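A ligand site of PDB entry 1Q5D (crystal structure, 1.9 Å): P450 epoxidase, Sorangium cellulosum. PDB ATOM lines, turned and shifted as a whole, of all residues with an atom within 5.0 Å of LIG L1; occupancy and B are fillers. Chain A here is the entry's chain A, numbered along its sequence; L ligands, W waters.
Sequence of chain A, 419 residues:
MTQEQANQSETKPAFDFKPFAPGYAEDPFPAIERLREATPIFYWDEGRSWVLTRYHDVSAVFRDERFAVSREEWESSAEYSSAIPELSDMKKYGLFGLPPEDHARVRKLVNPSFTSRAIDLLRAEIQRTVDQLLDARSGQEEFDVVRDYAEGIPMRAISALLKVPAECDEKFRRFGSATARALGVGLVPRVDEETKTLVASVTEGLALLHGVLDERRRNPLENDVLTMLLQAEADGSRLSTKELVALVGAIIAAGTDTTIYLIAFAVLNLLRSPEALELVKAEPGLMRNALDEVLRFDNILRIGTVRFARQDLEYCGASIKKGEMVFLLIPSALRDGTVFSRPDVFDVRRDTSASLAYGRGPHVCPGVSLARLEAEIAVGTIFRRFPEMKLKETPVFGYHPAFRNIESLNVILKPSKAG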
ATOM      1  N   ARG A  71      27.275 -30.842  14.034  1.00  0.00           N
ATOM      2  CA  ARG A  71      28.312 -31.571  14.745  1.00  0.00           C
ATOM      3  C   ARG A  71      28.895 -32.666  13.858  1.00  0.00           C
ATOM      4  O   ARG A  71      29.952 -33.215  14.169  1.00  0.00           O
ATOM      5  CB  ARG A  71      27.775 -32.134  16.063  1.00  0.00           C
ATOM      6  CG  ARG A  71      27.682 -31.119  17.194  1.00  0.00           C
ATOM      7  CD  ARG A  71      26.685 -29.991  16.941  1.00  0.00           C
ATOM      8  NE  ARG A  71      26.482 -29.142  18.127  1.00  0.00           N
ATOM      9  CZ  ARG A  71      26.506 -27.816  18.111  1.00  0.00           C
ATOM     10  NH1 ARG A  71      26.745 -27.166  16.987  1.00  0.00           N
ATOM     11  NH2 ARG A  71      26.301 -27.136  19.230  1.00  0.00           N
ATOM     12  N   MET A  90      17.486 -36.067  17.428  1.00  0.00           N
ATOM     13  CA  MET A  90      17.546 -34.646  17.756  1.00  0.00           C
ATOM     14  C   MET A  90      18.821 -33.981  17.261  1.00  0.00           C
ATOM     15  O   MET A  90      18.828 -32.810  16.877  1.00  0.00           O
ATOM     16  CB  MET A  90      17.408 -34.402  19.248  1.00  0.00           C
ATOM     17  CG  MET A  90      17.210 -32.926  19.558  1.00  0.00           C
ATOM     18  SD  MET A  90      17.198 -32.516  21.285  1.00  0.00           S
ATOM     19  CE  MET A  90      15.581 -33.148  21.746  1.00  0.00           C
ATOM     20  N   LYS A  91      19.912 -34.749  17.285  1.00  0.00           N
ATOM     21  CA  LYS A  91      21.203 -34.229  16.846  1.00  0.00           C
ATOM     22  C   LYS A  91      21.222 -34.047  15.327  1.00  0.00           C
ATOM     23  O   LYS A  91      21.829 -33.107  14.808  1.00  0.00           O
ATOM     24  CB  LYS A  91      22.316 -35.183  17.269  1.00  0.00           C
ATOM     25  CG  LYS A  91      22.579 -35.220  18.787  1.00  0.00           C
ATOM     26  CD  LYS A  91      23.732 -36.198  19.086  1.00  0.00           C
ATOM     27  CE  LYS A  91      24.075 -36.210  20.562  1.00  0.00           C
ATOM     28  NZ  LYS A  91      25.043 -37.324  20.904  1.00  0.00           N
ATOM     29  N   GLY A  94      17.650 -31.931  14.336  1.00  0.00           N
ATOM     30  CA  GLY A  94      17.467 -30.705  15.095  1.00  0.00           C
ATOM     31  C   GLY A  94      18.133 -29.525  14.414  1.00  0.00           C
ATOM     32  O   GLY A  94      18.809 -29.682  13.410  1.00  0.00           O
ATOM     33  N   LEU A  95      17.946 -28.343  14.987  1.00  0.00           N
ATOM     34  CA  LEU A  95      18.423 -27.111  14.372  1.00  0.00           C
ATOM     35  C   LEU A  95      19.945 -27.022  14.272  1.00  0.00           C
ATOM     36  O   LEU A  95      20.458 -26.354  13.385  1.00  0.00           O
ATOM     37  CB  LEU A  95      17.849 -25.902  15.107  1.00  0.00           C
ATOM     38  CG  LEU A  95      16.350 -25.684  14.897  1.00  0.00           C
ATOM     39  CD1 LEU A  95      15.847 -24.576  15.766  1.00  0.00           C
ATOM     40  CD2 LEU A  95      16.064 -25.369  13.429  1.00  0.00           C
ATOM     41  N   PHE A  96      20.670 -27.697  15.155  1.00  0.00           N
ATOM     42  CA  PHE A  96      22.137 -27.696  15.080  1.00  0.00           C
ATOM     43  C   PHE A  96      22.681 -28.727  14.081  1.00  0.00           C
ATOM     44  O   PHE A  96      23.851 -28.660  13.680  1.00  0.00           O
ATOM     45  CB  PHE A  96      22.774 -27.940  16.456  1.00  0.00           C
ATOM     46  CG  PHE A  96      22.677 -26.783  17.401  1.00  0.00           C
ATOM     47  CD1 PHE A  96      23.031 -26.950  18.738  1.00  0.00           C
ATOM     48  CD2 PHE A  96      22.235 -25.534  16.971  1.00  0.00           C
ATOM     49  CE1 PHE A  96      22.950 -25.896  19.634  1.00  0.00           C
ATOM     50  CE2 PHE A  96      22.158 -24.462  17.874  1.00  0.00           C
ATOM     51  CZ  PHE A  96      22.501 -24.643  19.198  1.00  0.00           C
ATOM     52  N   THR A 179      18.318 -32.956  28.842  1.00  0.00           N
ATOM     53  CA  THR A 179      18.658 -32.954  27.435  1.00  0.00           C
ATOM     54  C   THR A 179      19.820 -32.001  27.146  1.00  0.00           C
ATOM     55  O   THR A 179      20.740 -32.347  26.418  1.00  0.00           O
ATOM     56  CB  THR A 179      17.441 -32.548  26.601  1.00  0.00           C
ATOM     57  OG1 THR A 179      16.494 -33.618  26.592  1.00  0.00           O
ATOM     58  CG2 THR A 179      17.826 -32.382  25.145  1.00  0.00           C
ATOM     59  N   ALA A 180      19.757 -30.809  27.716  1.00  0.00           N
ATOM     60  CA  ALA A 180      20.811 -29.821  27.472  1.00  0.00           C
ATOM     61  C   ALA A 180      22.194 -30.346  27.900  1.00  0.00           C
ATOM     62  O   ALA A 180      23.189 -30.181  27.172  1.00  0.00           O
ATOM     63  CB  ALA A 180      20.474 -28.492  28.126  1.00  0.00           C
ATOM     64  N   ARG A 181      22.246 -30.993  29.074  1.00  0.00           N
ATOM     65  CA  ARG A 181      23.476 -31.646  29.565  1.00  0.00           C
ATOM     66  C   ARG A 181      23.871 -32.855  28.722  1.00  0.00           C
ATOM     67  O   ARG A 181      25.056 -33.045  28.409  1.00  0.00           O
ATOM     68  CB  ARG A 181      23.290 -32.128  31.008  1.00  0.00           C
ATOM     69  CG  ARG A 181      23.331 -31.055  32.073  1.00  0.00           C
ATOM     70  CD  ARG A 181      23.032 -31.593  33.463  1.00  0.00           C
ATOM     71  NE  ARG A 181      23.577 -30.779  34.532  1.00  0.00           N
ATOM     72  CZ  ARG A 181      22.846 -30.050  35.362  1.00  0.00           C
ATOM     73  NH1 ARG A 181      21.522 -30.026  35.228  1.00  0.00           N
ATOM     74  NH2 ARG A 181      23.425 -29.331  36.302  1.00  0.00           N
ATOM     75  N   LEU A 183      23.283 -33.526  25.660  1.00  0.00           N
ATOM     76  CA  LEU A 183      23.794 -33.126  24.353  1.00  0.00           C
ATOM     77  C   LEU A 183      25.275 -32.771  24.427  1.00  0.00           C
ATOM     78  O   LEU A 183      25.954 -32.677  23.395  1.00  0.00           O
ATOM     79  CB  LEU A 183      22.982 -31.942  23.796  1.00  0.00           C
ATOM     80  CG  LEU A 183      21.612 -32.310  23.214  1.00  0.00           C
ATOM     81  CD1 LEU A 183      20.842 -31.045  22.788  1.00  0.00           C
ATOM     82  CD2 LEU A 183      21.699 -33.316  22.063  1.00  0.00           C
ATOM     83  N   GLY A 184      25.772 -32.571  25.631  1.00  0.00           N
ATOM     84  CA  GLY A 184      27.194 -32.268  25.806  1.00  0.00           C
ATOM     85  C   GLY A 184      28.098 -33.481  25.933  1.00  0.00           C
ATOM     86  O   GLY A 184      29.330 -33.337  25.884  1.00  0.00           O
ATOM     87  N   LEU A 187      30.920 -34.192  23.537  1.00  0.00           N
ATOM     88  CA  LEU A 187      31.119 -32.949  22.803  1.00  0.00           C
ATOM     89  C   LEU A 187      31.933 -31.983  23.645  1.00  0.00           C
ATOM     90  O   LEU A 187      32.929 -31.455  23.184  1.00  0.00           O
ATOM     91  CB  LEU A 187      29.782 -32.292  22.434  1.00  0.00           C
ATOM     92  CG  LEU A 187      29.796 -31.060  21.513  1.00  0.00           C
ATOM     93  CD1 LEU A 187      30.474 -29.883  22.165  1.00  0.00           C
ATOM     94  CD2 LEU A 187      30.417 -31.343  20.168  1.00  0.00           C
ATOM     95  N   VAL A 188      31.477 -31.739  24.876  1.00  0.00           N
ATOM     96  CA  VAL A 188      32.183 -30.855  25.807  1.00  0.00           C
ATOM     97  C   VAL A 188      32.701 -31.645  27.016  1.00  0.00           C
ATOM     98  O   VAL A 188      32.082 -32.623  27.443  1.00  0.00           O
ATOM     99  CB  VAL A 188      31.289 -29.659  26.260  1.00  0.00           C
ATOM    100  CG1 VAL A 188      30.815 -28.863  25.069  1.00  0.00           C
ATOM    101  CG2 VAL A 188      30.113 -30.131  27.070  1.00  0.00           C
ATOM    102  N   ALA A 250      13.986 -29.300  21.227  1.00  0.00           N
ATOM    103  CA  ALA A 250      15.060 -28.309  21.319  1.00  0.00           C
ATOM    104  C   ALA A 250      14.567 -27.014  21.966  1.00  0.00           C
ATOM    105  O   ALA A 250      15.257 -26.412  22.791  1.00  0.00           O
ATOM    106  CB  ALA A 250      15.673 -28.052  19.939  1.00  0.00           C
ATOM    107  N   ALA A 253      14.434 -27.696  25.700  1.00  0.00           N
ATOM    108  CA  ALA A 253      15.781 -27.816  26.253  1.00  0.00           C
ATOM    109  C   ALA A 253      16.584 -26.493  26.187  1.00  0.00           C
ATOM    110  O   ALA A 253      17.409 -26.185  27.055  1.00  0.00           O
ATOM    111  CB  ALA A 253      16.537 -28.924  25.538  1.00  0.00           C
ATOM    112  N   ALA A 254      16.366 -25.722  25.132  1.00  0.00           N
ATOM    113  CA  ALA A 254      17.119 -24.487  24.954  1.00  0.00           C
ATOM    114  C   ALA A 254      16.553 -23.360  25.808  1.00  0.00           C
ATOM    115  O   ALA A 254      17.290 -22.441  26.204  1.00  0.00           O
ATOM    116  CB  ALA A 254      17.149 -24.074  23.482  1.00  0.00           C
ATOM    117  N   THR A 258      18.523 -21.702  30.403  1.00  0.00           N
ATOM    118  CA  THR A 258      18.989 -20.382  29.983  1.00  0.00           C
ATOM    119  C   THR A 258      18.162 -19.318  30.704  1.00  0.00           C
ATOM    120  O   THR A 258      18.709 -18.415  31.336  1.00  0.00           O
ATOM    121  CB  THR A 258      18.852 -20.234  28.457  1.00  0.00           C
ATOM    122  OG1 THR A 258      17.515 -20.552  28.063  1.00  0.00           O
ATOM    123  CG2 THR A 258      19.672 -21.300  27.743  1.00  0.00           C
ATOM    124  N   LEU A 301      26.944 -17.931  30.021  1.00  0.00           N
ATOM    125  CA  LEU A 301      27.661 -19.052  29.407  1.00  0.00           C
ATOM    126  C   LEU A 301      29.043 -19.212  30.043  1.00  0.00           C
ATOM    127  O   LEU A 301      29.762 -18.234  30.220  1.00  0.00           O
ATOM    128  CB  LEU A 301      27.833 -18.859  27.900  1.00  0.00           C
ATOM    129  CG  LEU A 301      26.528 -18.917  27.092  1.00  0.00           C
ATOM    130  CD1 LEU A 301      26.753 -18.702  25.587  1.00  0.00           C
ATOM    131  CD2 LEU A 301      25.873 -20.286  27.369  1.00  0.00           C
ATOM    132  N   GLY A 304      30.965 -20.729  25.877  1.00  0.00           N
ATOM    133  CA  GLY A 304      30.253 -20.078  24.802  1.00  0.00           C
ATOM    134  C   GLY A 304      29.543 -21.046  23.890  1.00  0.00           C
ATOM    135  O   GLY A 304      28.889 -21.985  24.348  1.00  0.00           O
ATOM    136  N   THR A 305      29.659 -20.828  22.592  1.00  0.00           N
ATOM    137  CA  THR A 305      29.049 -21.737  21.651  1.00  0.00           C
ATOM    138  C   THR A 305      30.113 -22.218  20.679  1.00  0.00           C
ATOM    139  O   THR A 305      31.235 -21.711  20.698  1.00  0.00           O
ATOM    140  CB  THR A 305      27.838 -21.109  20.944  1.00  0.00           C
ATOM    141  OG1 THR A 305      27.221 -22.113  20.134  1.00  0.00           O
ATOM    142  CG2 THR A 305      28.268 -20.032  19.947  1.00  0.00           C
ATOM    143  N   VAL A 306      29.776 -23.228  19.890  1.00  0.00           N
ATOM    144  CA  VAL A 306      30.770 -23.872  19.027  1.00  0.00           C
ATOM    145  C   VAL A 306      30.446 -23.783  17.544  1.00  0.00           C
ATOM    146  O   VAL A 306      29.285 -23.668  17.135  1.00  0.00           O
ATOM    147  CB  VAL A 306      30.960 -25.371  19.378  1.00  0.00           C
ATOM    148  CG1 VAL A 306      31.529 -25.510  20.765  1.00  0.00           C
ATOM    149  CG2 VAL A 306      29.651 -26.118  19.276  1.00  0.00           C
ATOM    150  N   PHE A 327      35.499 -22.816  19.736  1.00  0.00           N
ATOM    151  CA  PHE A 327      34.677 -22.189  20.753  1.00  0.00           C
ATOM    152  C   PHE A 327      34.734 -20.678  20.668  1.00  0.00           C
ATOM    153  O   PHE A 327      35.815 -20.086  20.606  1.00  0.00           O
ATOM    154  CB  PHE A 327      35.142 -22.617  22.146  1.00  0.00           C
ATOM    155  CG  PHE A 327      34.247 -23.621  22.820  1.00  0.00           C
ATOM    156  CD1 PHE A 327      34.653 -24.947  22.967  1.00  0.00           C
ATOM    157  CD2 PHE A 327      33.012 -23.233  23.342  1.00  0.00           C
ATOM    158  CE1 PHE A 327      33.825 -25.875  23.611  1.00  0.00           C
ATOM    159  CE2 PHE A 327      32.192 -24.165  23.992  1.00  0.00           C
ATOM    160  CZ  PHE A 327      32.605 -25.484  24.120  1.00  0.00           C
ATOM    161  N   PRO A 401      28.236 -27.978  32.353  1.00  0.00           N
ATOM    162  CA  PRO A 401      29.180 -27.894  31.226  1.00  0.00           C
ATOM    163  C   PRO A 401      28.976 -26.684  30.324  1.00  0.00           C
ATOM    164  O   PRO A 401      29.927 -26.279  29.646  1.00  0.00           O
ATOM    165  CB  PRO A 401      28.900 -29.175  30.435  1.00  0.00           C
ATOM    166  CG  PRO A 401      27.536 -29.606  30.849  1.00  0.00           C
ATOM    167  CD  PRO A 401      27.400 -29.191  32.295  1.00  0.00           C
ATOM    168  N   ALA A 402      27.769 -26.113  30.326  1.00  0.00           N
ATOM    169  CA  ALA A 402      27.498 -24.974  29.441  1.00  0.00           C
ATOM    170  C   ALA A 402      27.287 -23.642  30.166  1.00  0.00           C
ATOM    171  O   ALA A 402      27.494 -22.582  29.587  1.00  0.00           O
ATOM    172  CB  ALA A 402      26.269 -25.282  28.541  1.00  0.00           C
ATOM    173  N   PHE A 403      26.843 -23.692  31.416  1.00  0.00           N
ATOM    174  CA  PHE A 403      26.446 -22.483  32.098  1.00  0.00           C
ATOM    175  C   PHE A 403      27.247 -22.236  33.345  1.00  0.00           C
ATOM    176  O   PHE A 403      27.681 -23.178  34.020  1.00  0.00           O
ATOM    177  CB  PHE A 403      24.970 -22.578  32.517  1.00  0.00           C
ATOM    178  CG  PHE A 403      24.018 -22.728  31.369  1.00  0.00           C
ATOM    179  CD1 PHE A 403      23.214 -23.860  31.260  1.00  0.00           C
ATOM    180  CD2 PHE A 403      23.901 -21.718  30.410  1.00  0.00           C
ATOM    181  CE1 PHE A 403      22.334 -23.994  30.203  1.00  0.00           C
ATOM    182  CE2 PHE A 403      23.009 -21.841  29.357  1.00  0.00           C
ATOM    183  CZ  PHE A 403      22.231 -22.987  29.243  1.00  0.00           C
HETATM  184  O1  LIG L   1      21.885 -25.733  26.933  1.00  0.00           O
HETATM  185  C1  LIG L   1      23.253 -21.270  25.740  1.00  0.00           C
HETATM  186  O2  LIG L   1      20.962 -21.321  24.358  1.00  0.00           O
HETATM  187  C2  LIG L   1      22.305 -21.651  24.674  1.00  0.00           C
HETATM  188  C3  LIG L   1      21.074 -22.714  24.698  1.00  0.00           C
HETATM  189  C4  LIG L   1      22.558 -25.889  25.983  1.00  0.00           C
HETATM  190  O3  LIG L   1      22.183 -25.641  24.670  1.00  0.00           O
HETATM  191  C5  LIG L   1      20.770 -25.136  24.279  1.00  0.00           C
HETATM  192  C6  LIG L   1      20.915 -23.690  23.664  1.00  0.00           C
HETATM  193  C7  LIG L   1      20.326 -26.225  23.221  1.00  0.00           C
HETATM  194  C8  LIG L   1      20.043 -27.565  23.878  1.00  0.00           C
HETATM  195  C9  LIG L   1      20.210 -25.962  21.886  1.00  0.00           C
HETATM  196  C10 LIG L   1      19.865 -26.803  20.738  1.00  0.00           C
HETATM  197  N1  LIG L   1      20.269 -28.129  20.726  1.00  0.00           N
HETATM  198  C11 LIG L   1      19.881 -28.746  19.584  1.00  0.00           C
HETATM  199  C12 LIG L   1      20.199 -30.187  19.403  1.00  0.00           C
HETATM  200  C13 LIG L   1      19.229 -26.417  19.610  1.00  0.00           C
HETATM  201  S1  LIG L   1      19.085 -27.723  18.520  1.00  0.00           S
HETATM  202  C14 LIG L   1      24.007 -26.428  26.117  1.00  0.00           C
HETATM  203  C15 LIG L   1      24.425 -27.554  25.057  1.00  0.00           C
HETATM  204  O4  LIG L   1      23.388 -28.518  25.182  1.00  0.00           O
HETATM  205  C16 LIG L   1      25.939 -28.136  25.189  1.00  0.00           C
HETATM  206  C17 LIG L   1      26.080 -28.844  26.582  1.00  0.00           C
HETATM  207  C18 LIG L   1      26.154 -29.233  24.148  1.00  0.00           C
HETATM  208  C19 LIG L   1      27.056 -26.952  25.107  1.00  0.00           C
HETATM  209  O5  LIG L   1      27.856 -26.750  26.085  1.00  0.00           O
HETATM  210  C20 LIG L   1      27.262 -25.976  23.893  1.00  0.00           C
HETATM  211  C21 LIG L   1      28.781 -26.017  23.602  1.00  0.00           C
HETATM  212  C22 LIG L   1      26.415 -24.770  24.137  1.00  0.00           C
HETATM  213  O6  LIG L   1      26.996 -23.950  25.201  1.00  0.00           O
HETATM  214  C23 LIG L   1      26.360 -24.004  22.829  1.00  0.00           C
HETATM  215  C24 LIG L   1      25.683 -24.820  21.826  1.00  0.00           C
HETATM  216  C25 LIG L   1      25.492 -22.792  22.823  1.00  0.00           C
HETATM  217  C26 LIG L   1      24.657 -22.533  24.135  1.00  0.00           C
HETATM  218  C27 LIG L   1      23.171 -22.485  23.498  1.00  0.00           C
HETATM  219  C1  LG2 L   2      19.804 -20.571  19.958  1.00  0.00           C
HETATM  220  C2  LG2 L   2      20.975 -17.950  23.831  1.00  0.00           C
HETATM  221  C3  LG2 L   2      16.430 -18.418  25.515  1.00  0.00           C
HETATM  222  C4  LG2 L   2      15.461 -21.509  21.958  1.00  0.00           C
HETATM  223  C5  LG2 L   2      20.482 -19.742  20.821  1.00  0.00           C
HETATM  224  C6  LG2 L   2      21.810 -19.211  20.608  1.00  0.00           C
HETATM  225  C7  LG2 L   2      22.144 -18.504  21.686  1.00  0.00           C
HETATM  226  C8  LG2 L   2      21.034 -18.563  22.609  1.00  0.00           C
HETATM  227  C9  LG2 L   2      23.477 -17.741  21.901  1.00  0.00           C
HETATM  228  C10 LG2 L   2      22.675 -19.441  19.346  1.00  0.00           C
HETATM  229  C11 LG2 L   2      23.685 -20.560  19.573  1.00  0.00           C
HETATM  230  C12 LG2 L   2      24.575 -20.693  18.358  1.00  0.00           C
HETATM  231  O1  LG2 L   2      25.408 -21.652  18.297  1.00  0.00           O
HETATM  232  O2  LG2 L   2      24.464 -19.838  17.428  1.00  0.00           O
HETATM  233  C13 LG2 L   2      19.841 -17.872  24.587  1.00  0.00           C
HETATM  234  C14 LG2 L   2      19.760 -17.133  25.829  1.00  0.00           C
HETATM  235  C15 LG2 L   2      18.531 -17.272  26.300  1.00  0.00           C
HETATM  236  C16 LG2 L   2      17.771 -18.098  25.385  1.00  0.00           C
HETATM  237  C17 LG2 L   2      20.902 -16.341  26.519  1.00  0.00           C
HETATM  238  C18 LG2 L   2      18.086 -16.591  27.608  1.00  0.00           C
HETATM  239  C19 LG2 L   2      17.031 -17.022  28.290  1.00  0.00           C
HETATM  240  C20 LG2 L   2      15.744 -19.259  24.686  1.00  0.00           C
HETATM  241  C21 LG2 L   2      14.351 -19.623  24.784  1.00  0.00           C
HETATM  242  C22 LG2 L   2      14.098 -20.480  23.797  1.00  0.00           C
HETATM  243  C23 LG2 L   2      15.321 -20.671  23.034  1.00  0.00           C
HETATM  244  C24 LG2 L   2      13.392 -19.062  25.865  1.00  0.00           C
HETATM  245  C25 LG2 L   2      12.791 -21.197  23.403  1.00  0.00           C
HETATM  246  C26 LG2 L   2      11.620 -20.816  23.915  1.00  0.00           C
HETATM  247  C27 LG2 L   2      16.564 -21.580  21.143  1.00  0.00           C
HETATM  248  C28 LG2 L   2      16.667 -22.501  20.042  1.00  0.00           C
HETATM  249  C29 LG2 L   2      18.009 -22.221  19.415  1.00  0.00           C
HETATM  250  C30 LG2 L   2      18.590 -21.168  20.200  1.00  0.00           C
HETATM  251  C31 LG2 L   2      15.621 -23.540  19.596  1.00  0.00           C
HETATM  252  C32 LG2 L   2      18.618 -22.893  18.173  1.00  0.00           C
HETATM  253  C33 LG2 L   2      18.463 -21.871  17.036  1.00  0.00           C
HETATM  254  C34 LG2 L   2      19.058 -22.393  15.754  1.00  0.00           C
HETATM  255  O3  LG2 L   2      20.061 -23.147  15.838  1.00  0.00           O
HETATM  256  O4  LG2 L   2      18.519 -22.079  14.651  1.00  0.00           O
HETATM  257  N1  LG2 L   2      20.025 -19.330  22.044  1.00  0.00           N
HETATM  258  N2  LG2 L   2      18.604 -18.466  24.319  1.00  0.00           N
HETATM  259  N3  LG2 L   2      16.299 -19.927  23.620  1.00  0.00           N
HETATM  260  N4  LG2 L   2      17.709 -20.813  21.214  1.00  0.00           N
HETATM  261 FE1  LG2 L   2      18.111 -19.489  22.739  1.00  0.00          FE
HETATM  262  O   HOH W   1      30.062 -25.291  26.942  1.00  0.00           O
HETATM  263  O   HOH W   2      20.698 -30.629  16.149  1.00  0.00           O
HETATM  264  O   HOH W   3      24.954 -29.036  21.248  1.00  0.00           O
HETATM  265  O   HOH W   4      19.357 -24.477  27.981  1.00  0.00           O
HETATM  266  O   HOH W   5      22.920 -28.108  22.204  1.00  0.00           O
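Merely in contact with LIG L1: Leu 301 (3.2 Å), Thr 305 (3.3 Å), Ala 402 (3.3 Å), Leu 183 (3.5 Å), Arg 71 (3.5 Å), Phe 403 (3.6 Å), Gly 184 (3.6 Å), Thr 258 (3.6 Å), Ala 250 (3.7 Å), Ala 254 (3.8 Å), Val 188 (3.8 Å), Met 90 (3.9 Å), Phe 327 (3.9 Å) and Val 306 (3.98 Å).
Hydrophobic or aromatic side chains that line LIG L1: Phe 96, Ala 180, Leu 183, Val 188, Ala 250, Ala 254, Leu 301, Val 306, Phe 327, Ala 402 and Phe 403.
Within 4 Å of LIG L1: Arg 71, Met 90, Leu 95, Phe 96, Ala 180, Leu 183, Gly 184, Val 188, Ala 250, Ala 254, Thr 258, Leu 301, Gly 304, Thr 305, Val 306, Phe 327, Ala 402 and Phe 403.
The nearest printed residue that does not touch LIG L1 is Ala 253 (4.1 Å).
Water W1 bridges an oxygen (O5) of LIG L1 (2.8 Å) and the backbone carbonyl oxygen (O) of Pro 401 (2.9 Å).
O1 of LG2 L2 is in hydrogen-bond range of OG1 of Thr 305 (2.6 Å).
O of Gly 304 is in hydrogen-bond range of O6 of LIG L1, 2.9 Å away.
An oxygen (O4) of LIG L1 is in hydrogen-bond range of the backbone carbonyl oxygen (O) of Ala 180.
The backbone NH (N) of Phe 96 lies close to a sulfur (S1) of LIG L1 (3.7 Å).
A sulfur (S1) of LIG L1 lies close to the backbone NH (N) of Leu 95, 3.8 Å away.
OG1 of Thr 258 lies within hydrogen-bond range of O of Ala 254 (2.7 Å).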
